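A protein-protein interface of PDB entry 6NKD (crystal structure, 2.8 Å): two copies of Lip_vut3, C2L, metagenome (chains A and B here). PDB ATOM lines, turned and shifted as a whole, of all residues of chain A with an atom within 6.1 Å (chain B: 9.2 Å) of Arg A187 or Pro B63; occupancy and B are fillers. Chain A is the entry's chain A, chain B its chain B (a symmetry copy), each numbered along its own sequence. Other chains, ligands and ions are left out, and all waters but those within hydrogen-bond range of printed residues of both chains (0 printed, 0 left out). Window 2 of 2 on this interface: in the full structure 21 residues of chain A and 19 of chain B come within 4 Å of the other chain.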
ATOM      1  N   PRO A 139      13.806   0.098 -23.507  1.00  0.00           N
ATOM      2  CA  PRO A 139      13.779  -0.783 -22.330  1.00  0.00           C
ATOM      3  C   PRO A 139      12.865  -1.985 -22.490  1.00  0.00           C
ATOM      4  O   PRO A 139      12.945  -2.911 -21.673  1.00  0.00           O
ATOM      5  CB  PRO A 139      13.287   0.143 -21.213  1.00  0.00           C
ATOM      6  CG  PRO A 139      12.434   1.140 -21.920  1.00  0.00           C
ATOM      7  CD  PRO A 139      13.058   1.347 -23.280  1.00  0.00           C
ATOM      8  N   PHE A 140      12.008  -2.007 -23.514  1.00  0.00           N
ATOM      9  CA  PHE A 140      11.082  -3.110 -23.759  1.00  0.00           C
ATOM     10  C   PHE A 140      11.395  -3.713 -25.119  1.00  0.00           C
ATOM     11  O   PHE A 140      10.724  -3.403 -26.121  1.00  0.00           O
ATOM     12  CB  PHE A 140       9.632  -2.640 -23.673  1.00  0.00           C
ATOM     13  CG  PHE A 140       9.318  -1.881 -22.418  1.00  0.00           C
ATOM     14  CD1 PHE A 140       9.344  -2.513 -21.185  1.00  0.00           C
ATOM     15  CD2 PHE A 140       8.993  -0.536 -22.471  1.00  0.00           C
ATOM     16  CE1 PHE A 140       9.054  -1.816 -20.028  1.00  0.00           C
ATOM     17  CE2 PHE A 140       8.702   0.166 -21.317  1.00  0.00           C
ATOM     18  CZ  PHE A 140       8.732  -0.475 -20.094  1.00  0.00           C
ATOM     19  N   LEU A 183      19.582  -2.438 -16.994  1.00  0.00           N
ATOM     20  CA  LEU A 183      18.421  -1.746 -16.455  1.00  0.00           C
ATOM     21  C   LEU A 183      18.259  -2.075 -14.976  1.00  0.00           C
ATOM     22  O   LEU A 183      18.670  -3.141 -14.510  1.00  0.00           O
ATOM     23  CB  LEU A 183      17.148  -2.122 -17.216  1.00  0.00           C
ATOM     24  CG  LEU A 183      17.102  -1.732 -18.695  1.00  0.00           C
ATOM     25  CD1 LEU A 183      15.754  -2.094 -19.299  1.00  0.00           C
ATOM     26  CD2 LEU A 183      17.397  -0.251 -18.876  1.00  0.00           C
ATOM     27  N   SER A 184      17.648  -1.149 -14.243  1.00  0.00           N
ATOM     28  CA  SER A 184      17.526  -1.271 -12.797  1.00  0.00           C
ATOM     29  C   SER A 184      16.278  -2.084 -12.452  1.00  0.00           C
ATOM     30  O   SER A 184      15.746  -2.820 -13.288  1.00  0.00           O
ATOM     31  CB  SER A 184      17.517   0.120 -12.156  1.00  0.00           C
ATOM     32  OG  SER A 184      16.384   0.862 -12.570  1.00  0.00           O
ATOM     33  N   ILE A 185      15.793  -1.952 -11.215  1.00  0.00           N
ATOM     34  CA  ILE A 185      14.692  -2.787 -10.745  1.00  0.00           C
ATOM     35  C   ILE A 185      13.378  -2.398 -11.418  1.00  0.00           C
ATOM     36  O   ILE A 185      12.491  -3.242 -11.594  1.00  0.00           O
ATOM     37  CB  ILE A 185      14.603  -2.703  -9.208  1.00  0.00           C
ATOM     38  CG1 ILE A 185      13.560  -3.679  -8.659  1.00  0.00           C
ATOM     39  CG2 ILE A 185      14.311  -1.275  -8.763  1.00  0.00           C
ATOM     40  CD1 ILE A 185      13.966  -5.130  -8.773  1.00  0.00           C
ATOM     41  N   ASP A 186      13.231  -1.136 -11.820  1.00  0.00           N
ATOM     42  CA  ASP A 186      11.988  -0.672 -12.425  1.00  0.00           C
ATOM     43  C   ASP A 186      11.899  -0.969 -13.918  1.00  0.00           C
ATOM     44  O   ASP A 186      10.950  -0.515 -14.565  1.00  0.00           O
ATOM     45  CB  ASP A 186      11.802   0.828 -12.174  1.00  0.00           C
ATOM     46  CG  ASP A 186      12.891   1.681 -12.810  1.00  0.00           C
ATOM     47  OD1 ASP A 186      13.793   1.133 -13.480  1.00  0.00           O
ATOM     48  OD2 ASP A 186      12.839   2.916 -12.634  1.00  0.00           O
ATOM     49  N   ARG A 187      12.867  -1.695 -14.475  1.00  0.00           N
ATOM     50  CA  ARG A 187      12.878  -2.148 -15.864  1.00  0.00           C
ATOM     51  C   ARG A 187      12.864  -1.008 -16.876  1.00  0.00           C
ATOM     52  O   ARG A 187      12.694  -1.260 -18.075  1.00  0.00           O
ATOM     53  CB  ARG A 187      11.709  -3.099 -16.155  1.00  0.00           C
ATOM     54  CG  ARG A 187      11.875  -4.498 -15.588  1.00  0.00           C
ATOM     55  CD  ARG A 187      10.993  -4.716 -14.374  1.00  0.00           C
ATOM     56  NE  ARG A 187      10.970  -6.121 -13.974  1.00  0.00           N
ATOM     57  CZ  ARG A 187      11.799  -6.661 -13.087  1.00  0.00           C
ATOM     58  NH1 ARG A 187      12.721  -5.915 -12.494  1.00  0.00           N
ATOM     59  NH2 ARG A 187      11.703  -7.950 -12.790  1.00  0.00           N
ATOM     60  N   VAL A 188      13.031   0.240 -16.439  1.00  0.00           N
ATOM     61  CA  VAL A 188      13.030   1.368 -17.367  1.00  0.00           C
ATOM     62  C   VAL A 188      14.245   2.252 -17.110  1.00  0.00           C
ATOM     63  O   VAL A 188      14.801   2.844 -18.043  1.00  0.00           O
ATOM     64  CB  VAL A 188      11.724   2.181 -17.271  1.00  0.00           C
ATOM     65  CG1 VAL A 188      10.526   1.318 -17.636  1.00  0.00           C
ATOM     66  CG2 VAL A 188      11.552   2.759 -15.882  1.00  0.00           C
ATOM     67  N   HIS A 189      14.674   2.350 -15.834  1.00  0.00           N
ATOM     68  CA  HIS A 189      15.839   3.179 -15.574  1.00  0.00           C
ATOM     69  C   HIS A 189      17.101   2.325 -15.522  1.00  0.00           C
ATOM     70  O   HIS A 189      17.049   1.150 -15.147  1.00  0.00           O
ATOM     71  CB  HIS A 189      15.679   3.947 -14.258  1.00  0.00           C
ATOM     72  CG  HIS A 189      14.744   5.111 -14.355  1.00  0.00           C
ATOM     73  ND1 HIS A 189      13.432   5.052 -13.936  1.00  0.00           N
ATOM     74  CD2 HIS A 189      14.926   6.361 -14.842  1.00  0.00           C
ATOM     75  CE1 HIS A 189      12.849   6.218 -14.151  1.00  0.00           C
ATOM     76  NE2 HIS A 189      13.735   7.030 -14.701  1.00  0.00           N
ATOM     77  N   PHE B  46       3.878   3.366  -0.455  1.00  0.00           N
ATOM     78  CA  PHE B  46       5.061   3.677  -1.257  1.00  0.00           C
ATOM     79  C   PHE B  46       5.051   5.186  -1.485  1.00  0.00           C
ATOM     80  O   PHE B  46       4.334   5.680  -2.361  1.00  0.00           O
ATOM     81  CB  PHE B  46       5.061   2.917  -2.581  1.00  0.00           C
ATOM     82  CG  PHE B  46       5.068   1.423  -2.427  1.00  0.00           C
ATOM     83  CD1 PHE B  46       6.252   0.744  -2.188  1.00  0.00           C
ATOM     84  CD2 PHE B  46       3.893   0.696  -2.536  1.00  0.00           C
ATOM     85  CE1 PHE B  46       6.263  -0.631  -2.050  1.00  0.00           C
ATOM     86  CE2 PHE B  46       3.899  -0.678  -2.400  1.00  0.00           C
ATOM     87  CZ  PHE B  46       5.085  -1.343  -2.157  1.00  0.00           C
ATOM     88  N   LEU B  57       4.984   6.260 -12.466  1.00  0.00           N
ATOM     89  CA  LEU B  57       4.726   5.481 -13.671  1.00  0.00           C
ATOM     90  C   LEU B  57       5.832   4.466 -13.921  1.00  0.00           C
ATOM     91  O   LEU B  57       5.576   3.385 -14.464  1.00  0.00           O
ATOM     92  CB  LEU B  57       4.572   6.416 -14.871  1.00  0.00           C
ATOM     93  CG  LEU B  57       4.225   5.776 -16.214  1.00  0.00           C
ATOM     94  CD1 LEU B  57       2.935   4.980 -16.105  1.00  0.00           C
ATOM     95  CD2 LEU B  57       4.114   6.840 -17.295  1.00  0.00           C
ATOM     96  N   ALA B  58       7.063   4.785 -13.521  1.00  0.00           N
ATOM     97  CA  ALA B  58       8.166   3.843 -13.656  1.00  0.00           C
ATOM     98  C   ALA B  58       8.154   2.801 -12.544  1.00  0.00           C
ATOM     99  O   ALA B  58       8.530   1.646 -12.771  1.00  0.00           O
ATOM    100  CB  ALA B  58       9.495   4.596 -13.666  1.00  0.00           C
ATOM    101  N   MET B  59       7.732   3.194 -11.344  1.00  0.00           N
ATOM    102  CA  MET B  59       7.691   2.302 -10.189  1.00  0.00           C
ATOM    103  C   MET B  59       6.769   1.116 -10.404  1.00  0.00           C
ATOM    104  O   MET B  59       7.043   0.009  -9.937  1.00  0.00           O
ATOM    105  CB  MET B  59       7.234   3.060  -8.946  1.00  0.00           C
ATOM    106  CG  MET B  59       8.264   3.979  -8.335  1.00  0.00           C
ATOM    107  SD  MET B  59       7.365   5.271  -7.196  1.00  0.00           S
ATOM    108  CE  MET B  59       6.179   4.044  -6.254  1.00  0.00           C
ATOM    109  N   LEU B  60       5.663   1.360 -11.110  1.00  0.00           N
ATOM    110  CA  LEU B  60       4.657   0.329 -11.326  1.00  0.00           C
ATOM    111  C   LEU B  60       5.197  -0.871 -12.091  1.00  0.00           C
ATOM    112  O   LEU B  60       4.508  -1.892 -12.174  1.00  0.00           O
ATOM    113  CB  LEU B  60       3.454   0.928 -12.058  1.00  0.00           C
ATOM    114  CG  LEU B  60       2.710   2.033 -11.302  1.00  0.00           C
ATOM    115  CD1 LEU B  60       1.658   2.687 -12.186  1.00  0.00           C
ATOM    116  CD2 LEU B  60       2.076   1.486 -10.032  1.00  0.00           C
ATOM    117  N   ASN B  61       6.404  -0.777 -12.648  1.00  0.00           N
ATOM    118  CA  ASN B  61       7.062  -1.919 -13.260  1.00  0.00           C
ATOM    119  C   ASN B  61       7.885  -2.730 -12.270  1.00  0.00           C
ATOM    120  O   ASN B  61       8.302  -3.846 -12.603  1.00  0.00           O
ATOM    121  CB  ASN B  61       7.963  -1.462 -14.411  1.00  0.00           C
ATOM    122  CG  ASN B  61       7.177  -0.961 -15.603  1.00  0.00           C
ATOM    123  OD1 ASN B  61       6.853  -1.726 -16.511  1.00  0.00           O
ATOM    124  ND2 ASN B  61       6.867   0.330 -15.610  1.00  0.00           N
ATOM    125  N   GLU B  62       8.138  -2.203 -11.077  1.00  0.00           N
ATOM    126  CA  GLU B  62       8.871  -2.964 -10.073  1.00  0.00           C
ATOM    127  C   GLU B  62       8.025  -4.145  -9.616  1.00  0.00           C
ATOM    128  O   GLU B  62       6.850  -3.963  -9.276  1.00  0.00           O
ATOM    129  CB  GLU B  62       9.245  -2.081  -8.884  1.00  0.00           C
ATOM    130  CG  GLU B  62      10.234  -0.976  -9.219  1.00  0.00           C
ATOM    131  CD  GLU B  62      10.792  -0.301  -7.982  1.00  0.00           C
ATOM    132  OE1 GLU B  62      10.572  -0.826  -6.870  1.00  0.00           O
ATOM    133  OE2 GLU B  62      11.452   0.751  -8.121  1.00  0.00           O
ATOM    134  N   PRO B  63       8.578  -5.363  -9.596  1.00  0.00           N
ATOM    135  CA  PRO B  63       7.741  -6.544  -9.311  1.00  0.00           C
ATOM    136  C   PRO B  63       7.036  -6.495  -7.967  1.00  0.00           C
ATOM    137  O   PRO B  63       5.862  -6.877  -7.881  1.00  0.00           O
ATOM    138  CB  PRO B  63       8.741  -7.708  -9.387  1.00  0.00           C
ATOM    139  CG  PRO B  63      10.095  -7.083  -9.291  1.00  0.00           C
ATOM    140  CD  PRO B  63       9.970  -5.728  -9.902  1.00  0.00           C
ATOM    141  N   PHE B  64       7.710  -6.035  -6.913  1.00  0.00           N
ATOM    142  CA  PHE B  64       7.060  -5.987  -5.608  1.00  0.00           C
ATOM    143  C   PHE B  64       5.952  -4.942  -5.569  1.00  0.00           C
ATOM    144  O   PHE B  64       4.946  -5.133  -4.876  1.00  0.00           O
ATOM    145  CB  PHE B  64       8.089  -5.713  -4.512  1.00  0.00           C
ATOM    146  CG  PHE B  64       7.485  -5.581  -3.146  1.00  0.00           C
ATOM    147  CD1 PHE B  64       7.005  -6.695  -2.477  1.00  0.00           C
ATOM    148  CD2 PHE B  64       7.391  -4.343  -2.534  1.00  0.00           C
ATOM    149  CE1 PHE B  64       6.445  -6.577  -1.219  1.00  0.00           C
ATOM    150  CE2 PHE B  64       6.830  -4.218  -1.276  1.00  0.00           C
ATOM    151  CZ  PHE B  64       6.357  -5.336  -0.619  1.00  0.00           C
ATOM    152  N   ILE B  65       6.107  -3.842  -6.308  1.00  0.00           N
ATOM    153  CA  ILE B  65       5.097  -2.789  -6.286  1.00  0.00           C
ATOM    154  C   ILE B  65       3.856  -3.216  -7.062  1.00  0.00           C
ATOM    155  O   ILE B  65       2.724  -3.054  -6.593  1.00  0.00           O
ATOM    156  CB  ILE B  65       5.681  -1.475  -6.835  1.00  0.00           C
ATOM    157  CG1 ILE B  65       6.706  -0.897  -5.859  1.00  0.00           C
ATOM    158  CG2 ILE B  65       4.572  -0.467  -7.113  1.00  0.00           C
ATOM    159  CD1 ILE B  65       7.299   0.421  -6.309  1.00  0.00           C
ATOM    160  N   MET B  66       4.046  -3.775  -8.254  1.00  0.00           N
ATOM    161  CA  MET B  66       2.906  -4.144  -9.085  1.00  0.00           C
ATOM    162  C   MET B  66       2.163  -5.347  -8.503  1.00  0.00           C
ATOM    163  O   MET B  66       0.997  -5.577  -8.823  1.00  0.00           O
ATOM    164  CB  MET B  66       3.345  -4.426 -10.526  1.00  0.00           C
ATOM    165  CG  MET B  66       3.635  -5.879 -10.843  1.00  0.00           C
ATOM    166  SD  MET B  66       3.497  -6.236 -12.762  1.00  0.00           S
ATOM    167  CE  MET B  66       4.777  -4.925 -13.430  1.00  0.00           C
ATOM    168  N   GLU B  67       2.841  -6.110  -7.642  1.00  0.00           N
ATOM    169  CA  GLU B  67       2.150  -7.171  -6.914  1.00  0.00           C
ATOM    170  C   GLU B  67       1.157  -6.589  -5.918  1.00  0.00           C
ATOM    171  O   GLU B  67       0.023  -7.071  -5.808  1.00  0.00           O
ATOM    172  CB  GLU B  67       3.160  -8.070  -6.201  1.00  0.00           C
ATOM    173  CG  GLU B  67       3.787  -9.131  -7.090  1.00  0.00           C
ATOM    174  CD  GLU B  67       4.798  -9.983  -6.348  1.00  0.00           C
ATOM    175  OE1 GLU B  67       5.034  -9.715  -5.152  1.00  0.00           O
ATOM    176  OE2 GLU B  67       5.357 -10.919  -6.959  1.00  0.00           O
ATOM    177  N   GLN B  68       1.565  -5.551  -5.186  1.00  0.00           N
ATOM    178  CA  GLN B  68       0.651  -4.891  -4.262  1.00  0.00           C
ATOM    179  C   GLN B  68      -0.484  -4.199  -5.001  1.00  0.00           C
ATOM    180  O   GLN B  68      -1.611  -4.148  -4.496  1.00  0.00           O
ATOM    181  CB  GLN B  68       1.410  -3.882  -3.401  1.00  0.00           C
ATOM    182  CG  GLN B  68       2.647  -4.455  -2.738  1.00  0.00           C
ATOM    183  CD  GLN B  68       2.338  -5.682  -1.908  1.00  0.00           C
ATOM    184  OE1 GLN B  68       1.388  -5.695  -1.124  1.00  0.00           O
ATOM    185  NE2 GLN B  68       3.139  -6.729  -2.079  1.00  0.00           N
ATOM    186  N   VAL B  69      -0.209  -3.669  -6.194  1.00  0.00           N
ATOM    187  CA  VAL B  69      -1.250  -3.007  -6.969  1.00  0.00           C
ATOM    188  C   VAL B  69      -2.240  -4.027  -7.516  1.00  0.00           C
ATOM    189  O   VAL B  69      -3.452  -3.787  -7.527  1.00  0.00           O
ATOM    190  CB  VAL B  69      -0.624  -2.164  -8.094  1.00  0.00           C
ATOM    191  CG1 VAL B  69      -1.710  -1.581  -8.990  1.00  0.00           C
ATOM    192  CG2 VAL B  69       0.252  -1.061  -7.509  1.00  0.00           C
ATOM    193  N   LYS B  70      -1.743  -5.184  -7.965  1.00  0.00           N
ATOM    194  CA  LYS B  70      -2.618  -6.184  -8.573  1.00  0.00           C
ATOM    195  C   LYS B  70      -3.681  -6.668  -7.594  1.00  0.00           C
ATOM    196  O   LYS B  70      -4.834  -6.894  -7.980  1.00  0.00           O
ATOM    197  CB  LYS B  70      -1.787  -7.357  -9.097  1.00  0.00           C
ATOM    198  CG  LYS B  70      -2.495  -8.705  -9.042  1.00  0.00           C
ATOM    199  CD  LYS B  70      -1.896  -9.698 -10.025  1.00  0.00           C
ATOM    200  CE  LYS B  70      -2.359  -9.414 -11.446  1.00  0.00           C
ATOM    201  NZ  LYS B  70      -3.845  -9.458 -11.563  1.00  0.00           N
ATOM    202  N   LYS B 117      -1.579   1.987 -16.635  1.00  0.00           N
ATOM    203  CA  LYS B 117      -0.712   0.909 -16.172  1.00  0.00           C
ATOM    204  C   LYS B 117      -1.380   0.112 -15.057  1.00  0.00           C
ATOM    205  O   LYS B 117      -1.227  -1.112 -14.984  1.00  0.00           O
ATOM    206  CB  LYS B 117       0.627   1.472 -15.701  1.00  0.00           C
ATOM    207  CG  LYS B 117       1.653   0.409 -15.337  1.00  0.00           C
ATOM    208  CD  LYS B 117       2.813   0.402 -16.320  1.00  0.00           C
ATOM    209  CE  LYS B 117       3.733  -0.785 -16.090  1.00  0.00           C
ATOM    210  NZ  LYS B 117       3.067  -2.078 -16.410  1.00  0.00           N
ATOM    211  N   ILE B 121      -2.120  -3.964 -15.129  1.00  0.00           N
ATOM    212  CA  ILE B 121      -1.749  -4.886 -14.060  1.00  0.00           C
ATOM    213  C   ILE B 121      -2.986  -5.580 -13.504  1.00  0.00           C
ATOM    214  O   ILE B 121      -2.995  -6.799 -13.296  1.00  0.00           O
ATOM    215  CB  ILE B 121      -0.974  -4.141 -12.959  1.00  0.00           C
ATOM    216  CG1 ILE B 121       0.293  -3.506 -13.536  1.00  0.00           C
ATOM    217  CG2 ILE B 121      -0.634  -5.079 -11.810  1.00  0.00           C
ATOM    218  CD1 ILE B 121       0.983  -2.553 -12.588  1.00  0.00           C
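Arg A187 touches two residues of chain B. Pro B63 touches just these residues of chain A: Ile A185 (3.9 Å) and Arg A187 (3.8 Å). Of the printed residues of chain A, Ala B58 touches Asp A186 (3.4 Å), Val A188 (3.5 Å) and His A189 (3.8 Å). Of the printed residues of chain A, Asn B61 touches Asp A186 and Arg A187. Of the printed residues of chain B, Ile A185 touches Glu B62 (3.6 Å) and Pro B63 (3.9 Å). Printed residues of chain A within 4 Å of Glu B62: Ile A185 and Asp A186. Printed residues of chain B within 4 Å of His A189: Ala B58 (3.8 Å). Phe A140 touches none of the printed residues of chain B.
No position is printed for both chains. Of the 9 pairs that touch across the chains among the printed residues, none has its exchanged pair printed and touching as well.
Ile A185 touches Glu B62. Ile A185 touches Pro B63. Ala B58 touches Asp A186 (O to CB, 3.4 Å). O of Asp A186 touches CB of Asn B61, at 3.1 Å. Asp A186 touches Glu B62. Arg A187 touches Asn B61. NH1 of Arg A187 touches CD of Pro B63, 3.8 Å away. CB of Ala B58 touches CG2 of Val A188, 3.5 Å away. CE1 of His A189 touches CB of Ala B58, 3.8 Å away.
OG of Ser A184 is in hydrogen-bond range of OD1 of Asp A186 (2.8 Å). The guanidinium group of Arg A187 sits at hydrogen-bond distance from the backbone carbonyl oxygen of Ile A185 (2.8 Å). The side-chain carboxylate of Asp A186 sits at hydrogen-bond distance from a ring nitrogen (ND1) of His A189 (2.6 Å). O of His A189 is in hydrogen-bond range of N of Ser A184 (2.5 Å). OD1 of Asp A186 lies close to N of Val A188 (3.2 Å).
Of the 17 printed residues of chain B, 4 touch a printed residue of chain A. Printed residues of chain B that touch a printed residue of chain A: Ala B58, Asn B61, Glu B62 and Pro B63. Hydrophobic or aromatic side chains of chain B that line the printed part of chain A: Ala B58 and Pro B63. Hydrophobic or aromatic side chains of chain A that line the printed part of chain B: Ile A185, Val A188 and His A189. Among the printed residues, 9 pairs touch across the chains.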
